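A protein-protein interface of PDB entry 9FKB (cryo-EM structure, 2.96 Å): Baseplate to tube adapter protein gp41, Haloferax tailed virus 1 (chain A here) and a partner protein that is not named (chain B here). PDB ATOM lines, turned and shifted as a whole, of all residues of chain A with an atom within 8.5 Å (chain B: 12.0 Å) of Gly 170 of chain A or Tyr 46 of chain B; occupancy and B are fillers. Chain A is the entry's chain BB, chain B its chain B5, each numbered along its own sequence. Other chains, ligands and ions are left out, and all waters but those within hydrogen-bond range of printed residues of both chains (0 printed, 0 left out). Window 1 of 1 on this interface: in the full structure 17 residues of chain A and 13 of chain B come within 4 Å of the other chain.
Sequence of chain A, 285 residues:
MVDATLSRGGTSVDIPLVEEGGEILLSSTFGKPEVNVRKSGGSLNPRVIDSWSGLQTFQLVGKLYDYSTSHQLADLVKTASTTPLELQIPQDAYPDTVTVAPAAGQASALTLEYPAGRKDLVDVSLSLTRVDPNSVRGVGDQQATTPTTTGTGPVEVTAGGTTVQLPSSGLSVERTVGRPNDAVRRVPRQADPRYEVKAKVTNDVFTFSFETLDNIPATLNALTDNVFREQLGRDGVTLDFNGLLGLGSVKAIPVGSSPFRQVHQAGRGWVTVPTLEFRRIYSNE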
ATOM      1  N   TYR A 114      28.656  -5.572  23.419  1.00  0.00           N
ATOM      2  CA  TYR A 114      29.754  -5.517  22.471  1.00  0.00           C
ATOM      3  C   TYR A 114      29.154  -5.344  21.071  1.00  0.00           C
ATOM      4  O   TYR A 114      28.985  -6.318  20.327  1.00  0.00           O
ATOM      5  CB  TYR A 114      30.602  -6.782  22.632  1.00  0.00           C
ATOM      6  CG  TYR A 114      30.918  -7.175  24.059  1.00  0.00           C
ATOM      7  CD1 TYR A 114      30.067  -7.991  24.796  1.00  0.00           C
ATOM      8  CD2 TYR A 114      32.072  -6.714  24.680  1.00  0.00           C
ATOM      9  CE1 TYR A 114      30.370  -8.355  26.105  1.00  0.00           C
ATOM     10  CE2 TYR A 114      32.396  -7.068  25.985  1.00  0.00           C
ATOM     11  CZ  TYR A 114      31.544  -7.901  26.700  1.00  0.00           C
ATOM     12  OH  TYR A 114      31.885  -8.268  27.983  1.00  0.00           O
ATOM     13  N   PRO A 115      28.723  -4.112  20.697  1.00  0.00           N
ATOM     14  CA  PRO A 115      28.134  -3.878  19.376  1.00  0.00           C
ATOM     15  C   PRO A 115      29.215  -3.909  18.297  1.00  0.00           C
ATOM     16  O   PRO A 115      30.382  -3.633  18.565  1.00  0.00           O
ATOM     17  CB  PRO A 115      27.498  -2.487  19.477  1.00  0.00           C
ATOM     18  CG  PRO A 115      28.362  -1.809  20.505  1.00  0.00           C
ATOM     19  CD  PRO A 115      28.801  -2.874  21.489  1.00  0.00           C
ATOM     20  N   ALA A 116      28.820  -4.243  17.066  1.00  0.00           N
ATOM     21  CA  ALA A 116      29.743  -4.249  15.931  1.00  0.00           C
ATOM     22  C   ALA A 116      30.377  -2.869  15.683  1.00  0.00           C
ATOM     23  O   ALA A 116      29.728  -1.831  15.839  1.00  0.00           O
ATOM     24  CB  ALA A 116      29.016  -4.760  14.712  1.00  0.00           C
ATOM     25  N   GLY A 117      31.666  -2.852  15.301  1.00  0.00           N
ATOM     26  CA  GLY A 117      32.326  -1.637  14.843  1.00  0.00           C
ATOM     27  C   GLY A 117      33.005  -0.821  15.943  1.00  0.00           C
ATOM     28  O   GLY A 117      33.575   0.234  15.661  1.00  0.00           O
ATOM     29  N   ARG A 118      32.974  -1.323  17.181  1.00  0.00           N
ATOM     30  CA  ARG A 118      33.630  -0.722  18.336  1.00  0.00           C
ATOM     31  C   ARG A 118      34.666  -1.683  18.916  1.00  0.00           C
ATOM     32  O   ARG A 118      34.535  -2.904  18.824  1.00  0.00           O
ATOM     33  CB  ARG A 118      32.605  -0.329  19.402  1.00  0.00           C
ATOM     34  CG  ARG A 118      31.824   0.928  19.059  1.00  0.00           C
ATOM     35  CD  ARG A 118      30.838   1.181  20.186  1.00  0.00           C
ATOM     36  NE  ARG A 118      30.004   2.374  20.260  1.00  0.00           N
ATOM     37  CZ  ARG A 118      28.894   2.608  19.569  1.00  0.00           C
ATOM     38  NH1 ARG A 118      28.236   3.734  19.777  1.00  0.00           N
ATOM     39  NH2 ARG A 118      28.453   1.751  18.661  1.00  0.00           N
ATOM     40  N   PRO A 167      29.434 -16.679  11.952  1.00  0.00           N
ATOM     41  CA  PRO A 167      30.028 -15.696  11.051  1.00  0.00           C
ATOM     42  C   PRO A 167      30.196 -14.337  11.719  1.00  0.00           C
ATOM     43  O   PRO A 167      29.265 -13.779  12.280  1.00  0.00           O
ATOM     44  CB  PRO A 167      29.032 -15.653   9.882  1.00  0.00           C
ATOM     45  CG  PRO A 167      28.478 -17.056   9.863  1.00  0.00           C
ATOM     46  CD  PRO A 167      28.269 -17.330  11.336  1.00  0.00           C
ATOM     47  N   SER A 168      31.407 -13.783  11.603  1.00  0.00           N
ATOM     48  CA  SER A 168      31.828 -12.554  12.275  1.00  0.00           C
ATOM     49  C   SER A 168      31.086 -11.307  11.763  1.00  0.00           C
ATOM     50  O   SER A 168      31.008 -10.287  12.460  1.00  0.00           O
ATOM     51  CB  SER A 168      33.326 -12.410  12.165  1.00  0.00           C
ATOM     52  OG  SER A 168      33.706 -12.380  10.795  1.00  0.00           O
ATOM     53  N   SER A 169      30.558 -11.388  10.536  1.00  0.00           N
ATOM     54  CA  SER A 169      29.876 -10.317   9.815  1.00  0.00           C
ATOM     55  C   SER A 169      28.611  -9.826  10.529  1.00  0.00           C
ATOM     56  O   SER A 169      27.612 -10.535  10.600  1.00  0.00           O
ATOM     57  CB  SER A 169      29.594 -10.769   8.402  1.00  0.00           C
ATOM     58  OG  SER A 169      29.173 -12.127   8.367  1.00  0.00           O
ATOM     59  N   GLY A 170      28.659  -8.576  11.009  1.00  0.00           N
ATOM     60  CA  GLY A 170      27.567  -7.971  11.758  1.00  0.00           C
ATOM     61  C   GLY A 170      27.513  -8.437  13.215  1.00  0.00           C
ATOM     62  O   GLY A 170      26.681  -7.941  13.981  1.00  0.00           O
ATOM     63  N   LEU A 171      28.381  -9.394  13.595  1.00  0.00           N
ATOM     64  CA  LEU A 171      28.272 -10.078  14.882  1.00  0.00           C
ATOM     65  C   LEU A 171      28.377  -9.054  16.019  1.00  0.00           C
ATOM     66  O   LEU A 171      29.294  -8.234  16.054  1.00  0.00           O
ATOM     67  CB  LEU A 171      29.300 -11.220  14.970  1.00  0.00           C
ATOM     68  CG  LEU A 171      29.050 -12.260  16.065  1.00  0.00           C
ATOM     69  CD1 LEU A 171      29.693 -13.593  15.727  1.00  0.00           C
ATOM     70  CD2 LEU A 171      29.597 -11.829  17.407  1.00  0.00           C
ATOM     71  N   SER A 172      27.362  -9.081  16.895  1.00  0.00           N
ATOM     72  CA  SER A 172      27.172  -8.191  18.035  1.00  0.00           C
ATOM     73  C   SER A 172      26.694  -9.010  19.234  1.00  0.00           C
ATOM     74  O   SER A 172      25.779  -9.813  19.088  1.00  0.00           O
ATOM     75  CB  SER A 172      26.164  -7.122  17.687  1.00  0.00           C
ATOM     76  OG  SER A 172      26.584  -6.377  16.549  1.00  0.00           O
ATOM     77  N   VAL A 173      27.305  -8.818  20.413  1.00  0.00           N
ATOM     78  CA  VAL A 173      27.007  -9.604  21.612  1.00  0.00           C
ATOM     79  C   VAL A 173      26.356  -8.730  22.684  1.00  0.00           C
ATOM     80  O   VAL A 173      26.858  -7.661  23.009  1.00  0.00           O
ATOM     81  CB  VAL A 173      28.261 -10.297  22.194  1.00  0.00           C
ATOM     82  CG1 VAL A 173      27.972 -11.047  23.491  1.00  0.00           C
ATOM     83  CG2 VAL A 173      28.882 -11.259  21.197  1.00  0.00           C
ATOM     84  N   PHE A 208      23.365 -13.152  20.844  1.00  0.00           N
ATOM     85  CA  PHE A 208      24.062 -12.762  19.630  1.00  0.00           C
ATOM     86  C   PHE A 208      23.068 -12.242  18.597  1.00  0.00           C
ATOM     87  O   PHE A 208      21.942 -12.725  18.502  1.00  0.00           O
ATOM     88  CB  PHE A 208      24.735 -13.975  18.986  1.00  0.00           C
ATOM     89  CG  PHE A 208      25.790 -14.634  19.834  1.00  0.00           C
ATOM     90  CD1 PHE A 208      25.448 -15.622  20.750  1.00  0.00           C
ATOM     91  CD2 PHE A 208      27.126 -14.271  19.706  1.00  0.00           C
ATOM     92  CE1 PHE A 208      26.419 -16.247  21.525  1.00  0.00           C
ATOM     93  CE2 PHE A 208      28.100 -14.888  20.482  1.00  0.00           C
ATOM     94  CZ  PHE A 208      27.744 -15.873  21.387  1.00  0.00           C
ATOM     95  N   SER A 209      23.539 -11.317  17.763  1.00  0.00           N
ATOM     96  CA  SER A 209      22.974 -11.093  16.442  1.00  0.00           C
ATOM     97  C   SER A 209      24.107 -11.042  15.423  1.00  0.00           C
ATOM     98  O   SER A 209      25.169 -10.526  15.741  1.00  0.00           O
ATOM     99  CB  SER A 209      22.154  -9.837  16.407  1.00  0.00           C
ATOM    100  OG  SER A 209      21.595  -9.651  15.112  1.00  0.00           O
ATOM    101  N   PHE A 210      23.880 -11.598  14.224  1.00  0.00           N
ATOM    102  CA  PHE A 210      24.872 -11.693  13.160  1.00  0.00           C
ATOM    103  C   PHE A 210      24.191 -11.988  11.823  1.00  0.00           C
ATOM    104  O   PHE A 210      23.010 -12.308  11.786  1.00  0.00           O
ATOM    105  CB  PHE A 210      25.913 -12.766  13.486  1.00  0.00           C
ATOM    106  CG  PHE A 210      25.388 -14.160  13.762  1.00  0.00           C
ATOM    107  CD1 PHE A 210      24.988 -14.520  15.045  1.00  0.00           C
ATOM    108  CD2 PHE A 210      25.341 -15.129  12.760  1.00  0.00           C
ATOM    109  CE1 PHE A 210      24.535 -15.804  15.320  1.00  0.00           C
ATOM    110  CE2 PHE A 210      24.896 -16.416  13.033  1.00  0.00           C
ATOM    111  CZ  PHE A 210      24.490 -16.745  14.310  1.00  0.00           C
ATOM    112  N   GLU A 211      24.934 -11.880  10.714  1.00  0.00           N
ATOM    113  CA  GLU A 211      24.398 -12.237   9.405  1.00  0.00           C
ATOM    114  C   GLU A 211      25.317 -13.264   8.739  1.00  0.00           C
ATOM    115  O   GLU A 211      26.526 -13.067   8.669  1.00  0.00           O
ATOM    116  CB  GLU A 211      24.140 -10.985   8.564  1.00  0.00           C
ATOM    117  CG  GLU A 211      23.228 -10.008   9.286  1.00  0.00           C
ATOM    118  CD  GLU A 211      22.620  -8.858   8.491  1.00  0.00           C
ATOM    119  OE1 GLU A 211      22.808  -8.803   7.248  1.00  0.00           O
ATOM    120  OE2 GLU A 211      21.957  -7.999   9.116  1.00  0.00           O
ATOM    121  N   THR A 212      24.735 -14.387   8.286  1.00  0.00           N
ATOM    122  CA  THR A 212      25.486 -15.505   7.727  1.00  0.00           C
ATOM    123  C   THR A 212      25.620 -15.295   6.217  1.00  0.00           C
ATOM    124  O   THR A 212      24.609 -15.224   5.519  1.00  0.00           O
ATOM    125  CB  THR A 212      24.783 -16.833   8.043  1.00  0.00           C
ATOM    126  OG1 THR A 212      23.495 -16.848   7.422  1.00  0.00           O
ATOM    127  CG2 THR A 212      24.565 -17.072   9.518  1.00  0.00           C
ATOM    128  N   LEU A 213      26.866 -15.237   5.701  1.00  0.00           N
ATOM    129  CA  LEU A 213      27.124 -14.651   4.383  1.00  0.00           C
ATOM    130  C   LEU A 213      27.550 -15.634   3.282  1.00  0.00           C
ATOM    131  O   LEU A 213      27.495 -15.284   2.099  1.00  0.00           O
ATOM    132  CB  LEU A 213      28.146 -13.518   4.520  1.00  0.00           C
ATOM    133  CG  LEU A 213      27.714 -12.311   5.341  1.00  0.00           C
ATOM    134  CD1 LEU A 213      28.739 -11.210   5.150  1.00  0.00           C
ATOM    135  CD2 LEU A 213      26.308 -11.814   4.971  1.00  0.00           C
ATOM    136  N   VAL A 273      20.410 -13.292  11.519  1.00  0.00           N
ATOM    137  CA  VAL A 273      20.077 -13.856  12.824  1.00  0.00           C
ATOM    138  C   VAL A 273      19.787 -12.719  13.805  1.00  0.00           C
ATOM    139  O   VAL A 273      20.710 -12.166  14.401  1.00  0.00           O
ATOM    140  CB  VAL A 273      21.191 -14.794  13.328  1.00  0.00           C
ATOM    141  CG1 VAL A 273      20.911 -15.291  14.740  1.00  0.00           C
ATOM    142  CG2 VAL A 273      21.350 -15.981  12.390  1.00  0.00           C
ATOM    143  N   HIS B  42      23.720  -1.279  -0.392  1.00  0.00           N
ATOM    144  CA  HIS B  42      24.892  -1.847   0.267  1.00  0.00           C
ATOM    145  C   HIS B  42      24.672  -1.978   1.769  1.00  0.00           C
ATOM    146  O   HIS B  42      24.424  -0.983   2.449  1.00  0.00           O
ATOM    147  CB  HIS B  42      26.151  -0.984   0.018  1.00  0.00           C
ATOM    148  CG  HIS B  42      26.863  -1.318  -1.250  1.00  0.00           C
ATOM    149  ND1 HIS B  42      28.183  -0.957  -1.518  1.00  0.00           N
ATOM    150  CD2 HIS B  42      26.412  -2.014  -2.315  1.00  0.00           C
ATOM    151  CE1 HIS B  42      28.508  -1.400  -2.719  1.00  0.00           C
ATOM    152  NE2 HIS B  42      27.441  -2.063  -3.225  1.00  0.00           N
ATOM    153  N   ALA B  43      24.846  -3.204   2.272  1.00  0.00           N
ATOM    154  CA  ALA B  43      25.034  -3.459   3.688  1.00  0.00           C
ATOM    155  C   ALA B  43      26.536  -3.464   3.967  1.00  0.00           C
ATOM    156  O   ALA B  43      27.238  -4.317   3.433  1.00  0.00           O
ATOM    157  CB  ALA B  43      24.394  -4.786   4.045  1.00  0.00           C
ATOM    158  N   GLU B  44      27.013  -2.535   4.812  1.00  0.00           N
ATOM    159  CA  GLU B  44      28.378  -2.581   5.312  1.00  0.00           C
ATOM    160  C   GLU B  44      28.345  -3.108   6.743  1.00  0.00           C
ATOM    161  O   GLU B  44      27.682  -2.529   7.606  1.00  0.00           O
ATOM    162  CB  GLU B  44      29.042  -1.209   5.247  1.00  0.00           C
ATOM    163  CG  GLU B  44      29.318  -0.766   3.830  1.00  0.00           C
ATOM    164  CD  GLU B  44      30.123   0.514   3.706  1.00  0.00           C
ATOM    165  OE1 GLU B  44      29.613   1.583   4.119  1.00  0.00           O
ATOM    166  OE2 GLU B  44      31.253   0.452   3.182  1.00  0.00           O
ATOM    167  N   LEU B  45      29.051  -4.224   6.982  1.00  0.00           N
ATOM    168  CA  LEU B  45      28.944  -4.986   8.215  1.00  0.00           C
ATOM    169  C   LEU B  45      30.258  -4.939   8.978  1.00  0.00           C
ATOM    170  O   LEU B  45      31.319  -5.269   8.444  1.00  0.00           O
ATOM    171  CB  LEU B  45      28.541  -6.426   7.881  1.00  0.00           C
ATOM    172  CG  LEU B  45      27.229  -6.548   7.115  1.00  0.00           C
ATOM    173  CD1 LEU B  45      27.508  -6.898   5.661  1.00  0.00           C
ATOM    174  CD2 LEU B  45      26.234  -7.497   7.777  1.00  0.00           C
ATOM    175  N   TYR B  46      30.173  -4.527  10.254  1.00  0.00           N
ATOM    176  CA  TYR B  46      31.325  -4.462  11.150  1.00  0.00           C
ATOM    177  C   TYR B  46      31.359  -5.688  12.078  1.00  0.00           C
ATOM    178  O   TYR B  46      30.529  -6.584  11.939  1.00  0.00           O
ATOM    179  CB  TYR B  46      31.283  -3.122  11.887  1.00  0.00           C
ATOM    180  CG  TYR B  46      31.550  -1.932  10.994  1.00  0.00           C
ATOM    181  CD1 TYR B  46      30.573  -1.427  10.148  1.00  0.00           C
ATOM    182  CD2 TYR B  46      32.800  -1.337  10.954  1.00  0.00           C
ATOM    183  CE1 TYR B  46      30.828  -0.361   9.294  1.00  0.00           C
ATOM    184  CE2 TYR B  46      33.072  -0.275  10.103  1.00  0.00           C
ATOM    185  CZ  TYR B  46      32.083   0.224   9.272  1.00  0.00           C
ATOM    186  OH  TYR B  46      32.338   1.284   8.442  1.00  0.00           O
ATOM    187  N   THR B  47      32.292  -5.729  13.049  1.00  0.00           N
ATOM    188  CA  THR B  47      32.402  -6.871  13.966  1.00  0.00           C
ATOM    189  C   THR B  47      32.747  -6.449  15.405  1.00  0.00           C
ATOM    190  O   THR B  47      33.058  -5.297  15.641  1.00  0.00           O
ATOM    191  CB  THR B  47      33.289  -7.955  13.346  1.00  0.00           C
ATOM    192  OG1 THR B  47      32.996  -9.193  13.996  1.00  0.00           O
ATOM    193  CG2 THR B  47      34.769  -7.669  13.472  1.00  0.00           C
ATOM    194  N   ILE B  48      32.755  -7.386  16.374  1.00  0.00           N
ATOM    195  CA  ILE B  48      32.799  -7.085  17.809  1.00  0.00           C
ATOM    196  C   ILE B  48      34.110  -6.477  18.329  1.00  0.00           C
ATOM    197  O   ILE B  48      34.109  -5.942  19.439  1.00  0.00           O
ATOM    198  CB  ILE B  48      32.459  -8.341  18.642  1.00  0.00           C
ATOM    199  CG1 ILE B  48      33.376  -9.513  18.268  1.00  0.00           C
ATOM    200  CG2 ILE B  48      30.980  -8.663  18.547  1.00  0.00           C
ATOM    201  CD1 ILE B  48      33.038 -10.880  18.879  1.00  0.00           C
ATOM    202  N   ASP B  49      35.247  -6.648  17.628  1.00  0.00           N
ATOM    203  CA  ASP B  49      36.554  -6.273  18.168  1.00  0.00           C
ATOM    204  C   ASP B  49      37.432  -5.613  17.100  1.00  0.00           C
ATOM    205  O   ASP B  49      38.653  -5.815  17.059  1.00  0.00           O
ATOM    206  CB  ASP B  49      37.246  -7.450  18.873  1.00  0.00           C
ATOM    207  CG  ASP B  49      38.385  -7.077  19.823  1.00  0.00           C
ATOM    208  OD1 ASP B  49      38.441  -5.907  20.270  1.00  0.00           O
ATOM    209  OD2 ASP B  49      39.209  -7.973  20.134  1.00  0.00           O
ATOM    210  N   SER B  50      36.793  -4.794  16.258  1.00  0.00           N
ATOM    211  CA  SER B  50      37.469  -4.001  15.243  1.00  0.00           C
ATOM    212  C   SER B  50      36.648  -2.756  14.911  1.00  0.00           C
ATOM    213  O   SER B  50      35.425  -2.801  14.870  1.00  0.00           O
ATOM    214  CB  SER B  50      37.753  -4.817  14.007  1.00  0.00           C
ATOM    215  OG  SER B  50      38.339  -4.016  13.008  1.00  0.00           O
ATOM    216  N   THR B  51      37.346  -1.655  14.623  1.00  0.00           N
ATOM    217  CA  THR B  51      36.718  -0.456  14.084  1.00  0.00           C
ATOM    218  C   THR B  51      36.533  -0.544  12.567  1.00  0.00           C
ATOM    219  O   THR B  51      35.754   0.235  12.025  1.00  0.00           O
ATOM    220  CB  THR B  51      37.520   0.806  14.413  1.00  0.00           C
ATOM    221  OG1 THR B  51      38.789   0.728  13.748  1.00  0.00           O
ATOM    222  CG2 THR B  51      37.636   1.040  15.904  1.00  0.00           C
ATOM    223  N   PHE B  52      37.256  -1.449  11.891  1.00  0.00           N
ATOM    224  CA  PHE B  52      37.184  -1.584  10.441  1.00  0.00           C
ATOM    225  C   PHE B  52      35.948  -2.373  10.008  1.00  0.00           C
ATOM    226  O   PHE B  52      35.449  -3.234  10.728  1.00  0.00           O
ATOM    227  CB  PHE B  52      38.437  -2.274   9.902  1.00  0.00           C
ATOM    228  CG  PHE B  52      39.764  -1.551  10.029  1.00  0.00           C
ATOM    229  CD1 PHE B  52      39.872  -0.266  10.565  1.00  0.00           C
ATOM    230  CD2 PHE B  52      40.933  -2.202   9.647  1.00  0.00           C
ATOM    231  CE1 PHE B  52      41.111   0.363  10.668  1.00  0.00           C
ATOM    232  CE2 PHE B  52      42.172  -1.582   9.765  1.00  0.00           C
ATOM    233  CZ  PHE B  52      42.257  -0.299  10.272  1.00  0.00           C
ATOM    234  N   ARG B  53      35.488  -2.109   8.777  1.00  0.00           N
ATOM    235  CA  ARG B  53      34.444  -2.882   8.120  1.00  0.00           C
ATOM    236  C   ARG B  53      34.913  -4.322   7.927  1.00  0.00           C
ATOM    237  O   ARG B  53      36.018  -4.549   7.441  1.00  0.00           O
ATOM    238  CB  ARG B  53      34.114  -2.201   6.790  1.00  0.00           C
ATOM    239  CG  ARG B  53      32.866  -2.720   6.090  1.00  0.00           C
ATOM    240  CD  ARG B  53      32.727  -2.060   4.728  1.00  0.00           C
ATOM    241  NE  ARG B  53      33.699  -2.533   3.746  1.00  0.00           N
ATOM    242  CZ  ARG B  53      34.095  -1.877   2.653  1.00  0.00           C
ATOM    243  NH1 ARG B  53      34.977  -2.451   1.854  1.00  0.00           N
ATOM    244  NH2 ARG B  53      33.666  -0.643   2.415  1.00  0.00           N
ATOM    245  N   ASP B  54      34.077  -5.292   8.324  1.00  0.00           N
ATOM    246  CA  ASP B  54      34.421  -6.699   8.198  1.00  0.00           C
ATOM    247  C   ASP B  54      34.032  -7.236   6.818  1.00  0.00           C
ATOM    248  O   ASP B  54      34.834  -7.877   6.138  1.00  0.00           O
ATOM    249  CB  ASP B  54      33.785  -7.509   9.331  1.00  0.00           C
ATOM    250  CG  ASP B  54      34.383  -8.908   9.459  1.00  0.00           C
ATOM    251  OD1 ASP B  54      35.622  -9.055   9.274  1.00  0.00           O
ATOM    252  OD2 ASP B  54      33.613  -9.860   9.743  1.00  0.00           O
ATOM    253  N   GLU B  55      32.786  -6.964   6.398  1.00  0.00           N
ATOM    254  CA  GLU B  55      32.280  -7.370   5.086  1.00  0.00           C
ATOM    255  C   GLU B  55      31.305  -6.354   4.483  1.00  0.00           C
ATOM    256  O   GLU B  55      30.796  -5.463   5.172  1.00  0.00           O
ATOM    257  CB  GLU B  55      31.631  -8.751   5.159  1.00  0.00           C
ATOM    258  CG  GLU B  55      32.543  -9.889   4.706  1.00  0.00           C
ATOM    259  CD  GLU B  55      33.166  -9.751   3.321  1.00  0.00           C
ATOM    260  OE1 GLU B  55      32.819  -8.805   2.581  1.00  0.00           O
ATOM    261  OE2 GLU B  55      34.003 -10.616   2.973  1.00  0.00           O
ATOM    262  N   VAL B  56      31.051  -6.481   3.172  1.00  0.00           N
ATOM    263  CA  VAL B  56      30.071  -5.647   2.483  1.00  0.00           C
ATOM    264  C   VAL B  56      29.306  -6.474   1.447  1.00  0.00           C
ATOM    265  O   VAL B  56      29.912  -7.217   0.671  1.00  0.00           O
ATOM    266  CB  VAL B  56      30.705  -4.361   1.892  1.00  0.00           C
ATOM    267  CG1 VAL B  56      31.913  -4.615   0.989  1.00  0.00           C
ATOM    268  CG2 VAL B  56      29.685  -3.481   1.176  1.00  0.00           C
ATOM    269  N   LYS B  57      27.964  -6.305   1.413  1.00  0.00           N
ATOM    270  CA  LYS B  57      27.074  -7.068   0.542  1.00  0.00           C
ATOM    271  C   LYS B  57      26.058  -6.194  -0.199  1.00  0.00           C
ATOM    272  O   LYS B  57      25.497  -5.257   0.366  1.00  0.00           O
ATOM    273  CB  LYS B  57      26.333  -8.156   1.323  1.00  0.00           C
ATOM    274  CG  LYS B  57      27.194  -9.316   1.797  1.00  0.00           C
ATOM    275  CD  LYS B  57      27.700 -10.212   0.663  1.00  0.00           C
ATOM    276  CE  LYS B  57      28.569 -11.348   1.175  1.00  0.00           C
ATOM    277  NZ  LYS B  57      28.597 -12.563   0.305  1.00  0.00           N
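The backbone carbonyl oxygen (O) of Leu 213 of chain A sits at hydrogen-bond distance from the side-chain amino group (NZ) of Lys 57 of chain B (3.4 Å).
O of Arg 118 of chain A sits close to O of Ile 48 of chain B (3.1 Å).
O of Tyr 46 of chain B is in hydrogen-bond range of N of Gly 170 of chain A, at 2.9 Å.
The side-chain carboxylate of Asp 54 of chain B is in hydrogen-bond range of the side-chain hydroxyl of Ser 168 of chain A (2.7 Å).
O of Thr 47 of chain B is in hydrogen-bond range of N of Gly 117 of chain A, at 2.8 Å.
The backbone carbonyl oxygen of Ser 168 of chain A is in hydrogen-bond range of the side-chain hydroxyl of Thr 47 of chain B, at 2.7 Å.
OG of Ser 50 of chain B sits at hydrogen-bond distance from N of Phe 52 of chain B (3.0 Å).
O of Lys 57 of chain B sits at hydrogen-bond distance from N of Ala 43 of chain B.
The backbone NH (N) of Tyr 114 of chain A lies within hydrogen-bond range of the backbone carbonyl oxygen (O) of Val 173 of chain A, 2.8 Å away.
O of Ser 209 of chain A lies within hydrogen-bond range of N of Ser 172 of chain A (2.9 Å).
The backbone NH (N) of Leu 45 of chain B sits at hydrogen-bond distance from the backbone carbonyl oxygen (O) of Glu 55 of chain B.
The side-chain hydroxyl of Ser 169 of chain A is in hydrogen-bond range of the backbone carbonyl oxygen of Glu 211 of chain A, at 2.8 Å.
Among the printed residues, pairs that only touch across the chains: Leu 171 of chain A with Ile 48 of chain B (3.0 Å), Gly 117 of chain A with Ser 50 of chain B (3.3 Å), Gly 117 of chain A with Tyr 46 of chain B (3.4 Å), Ala 116 of chain A with Thr 47 of chain B (3.5 Å), Ser 169 of chain A with Asp 54 of chain B (3.5 Å), Tyr 114 of chain A with Ile 48 of chain B (3.6 Å), Gly 117 of chain A with Thr 51 of chain B (3.6 Å), Ala 116 of chain A with Tyr 46 of chain B (3.6 Å), Arg 118 of chain A with Ser 50 of chain B (3.7 Å), Glu 211 of chain A with Leu 45 of chain B (3.7 Å), Ser 168 of chain A with Tyr 46 of chain B (3.8 Å), Leu 213 of chain A with Glu 55 of chain B (3.8 Å), Gly 170 of chain A with Leu 45 of chain B (3.8 Å), Ser 172 of chain A with Ile 48 of chain B (3.9 Å), Leu 171 of chain A with Tyr 46 of chain B (3.9 Å), Leu 171 of chain A with Thr 47 of chain B (3.9 Å) and Arg 118 of chain A with Asp 49 of chain B (3.98 Å).
Of the printed residues of chain B, Gly 170 of chain A touches Leu 45 and Tyr 46.
Of chain A, only Ala 116 (3.6 Å), Gly 117 (3.4 Å), Ser 168 (3.8 Å), Gly 170 (2.9 Å) and Leu 171 (3.9 Å) come within 4 Å of Tyr 46 of chain B.
Ala 116 of chain A touches just these residues of chain B: Tyr 46 (3.6 Å) and Thr 47 (3.5 Å).
Of the printed residues of chain B, Gly 117 of chain A touches Tyr 46 (3.4 Å), Thr 47 (2.8 Å), Ser 50 (3.3 Å) and Thr 51 (3.6 Å).
Of chain B, only Tyr 46, Thr 47 and Asp 54 come within 4 Å of Ser 168 of chain A.
Of chain B, only Asp 54 (3.5 Å) comes within 4 Å of Ser 169 of chain A.
Of the printed residues of chain B, Ser 172 of chain A touches Ile 48 (3.9 Å).
No residue of chain B comes within 4 Å of Ser 209 of chain A.
Of chain B, only Leu 45 (3.7 Å) comes within 4 Å of Glu 211 of chain A.
Printed residues of chain A within 4 Å of Thr 47 of chain B: Ala 116 (3.5 Å), Gly 117 (2.8 Å), Ser 168 (2.7 Å) and Leu 171 (3.9 Å).
Of the printed residues of chain B, Tyr 114 of chain A touches Ile 48 (3.6 Å).
Of the printed residues of chain A, Glu 55 of chain B touches Leu 213.
The nearest residue of chain B that does not touch Gly 170 of chain A is Thr 47 of chain B (5.0 Å).
The nearest printed residue of chain B that does not touch Arg 118 of chain A is Thr 47 of chain B (4.2 Å).
Of the 16 printed residues of chain B, 10 touch a printed residue of chain A.
Printed residues of chain B that touch a printed residue of chain A: Leu 45, Tyr 46, Thr 47, Ile 48, Asp 49, Ser 50, Thr 51, Asp 54, Glu 55 and Lys 57.
Hydrophobic or aromatic side chains of chain B within 4 Å of the printed part of chain A: Leu 45, Tyr 46 and Ile 48.
Printed residues of chain A that touch a printed residue of chain B: Tyr 114, Ala 116, Gly 117, Arg 118, Ser 168, Ser 169, Gly 170, Leu 171, Ser 172, Glu 211 and Leu 213.
Hydrophobic or aromatic side chains of chain A that line the printed part of chain B: Ala 116, Leu 171 and Leu 213.
Along chain A the printed residues that touch a printed residue of chain B span positions 114 to 213.
Among the printed residues, 23 pairs touch across the chains.
Among the printed residues, no Asp or Glu carboxylate lies within 4 Å of a Lys or Arg side-chain nitrogen of the other chain.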
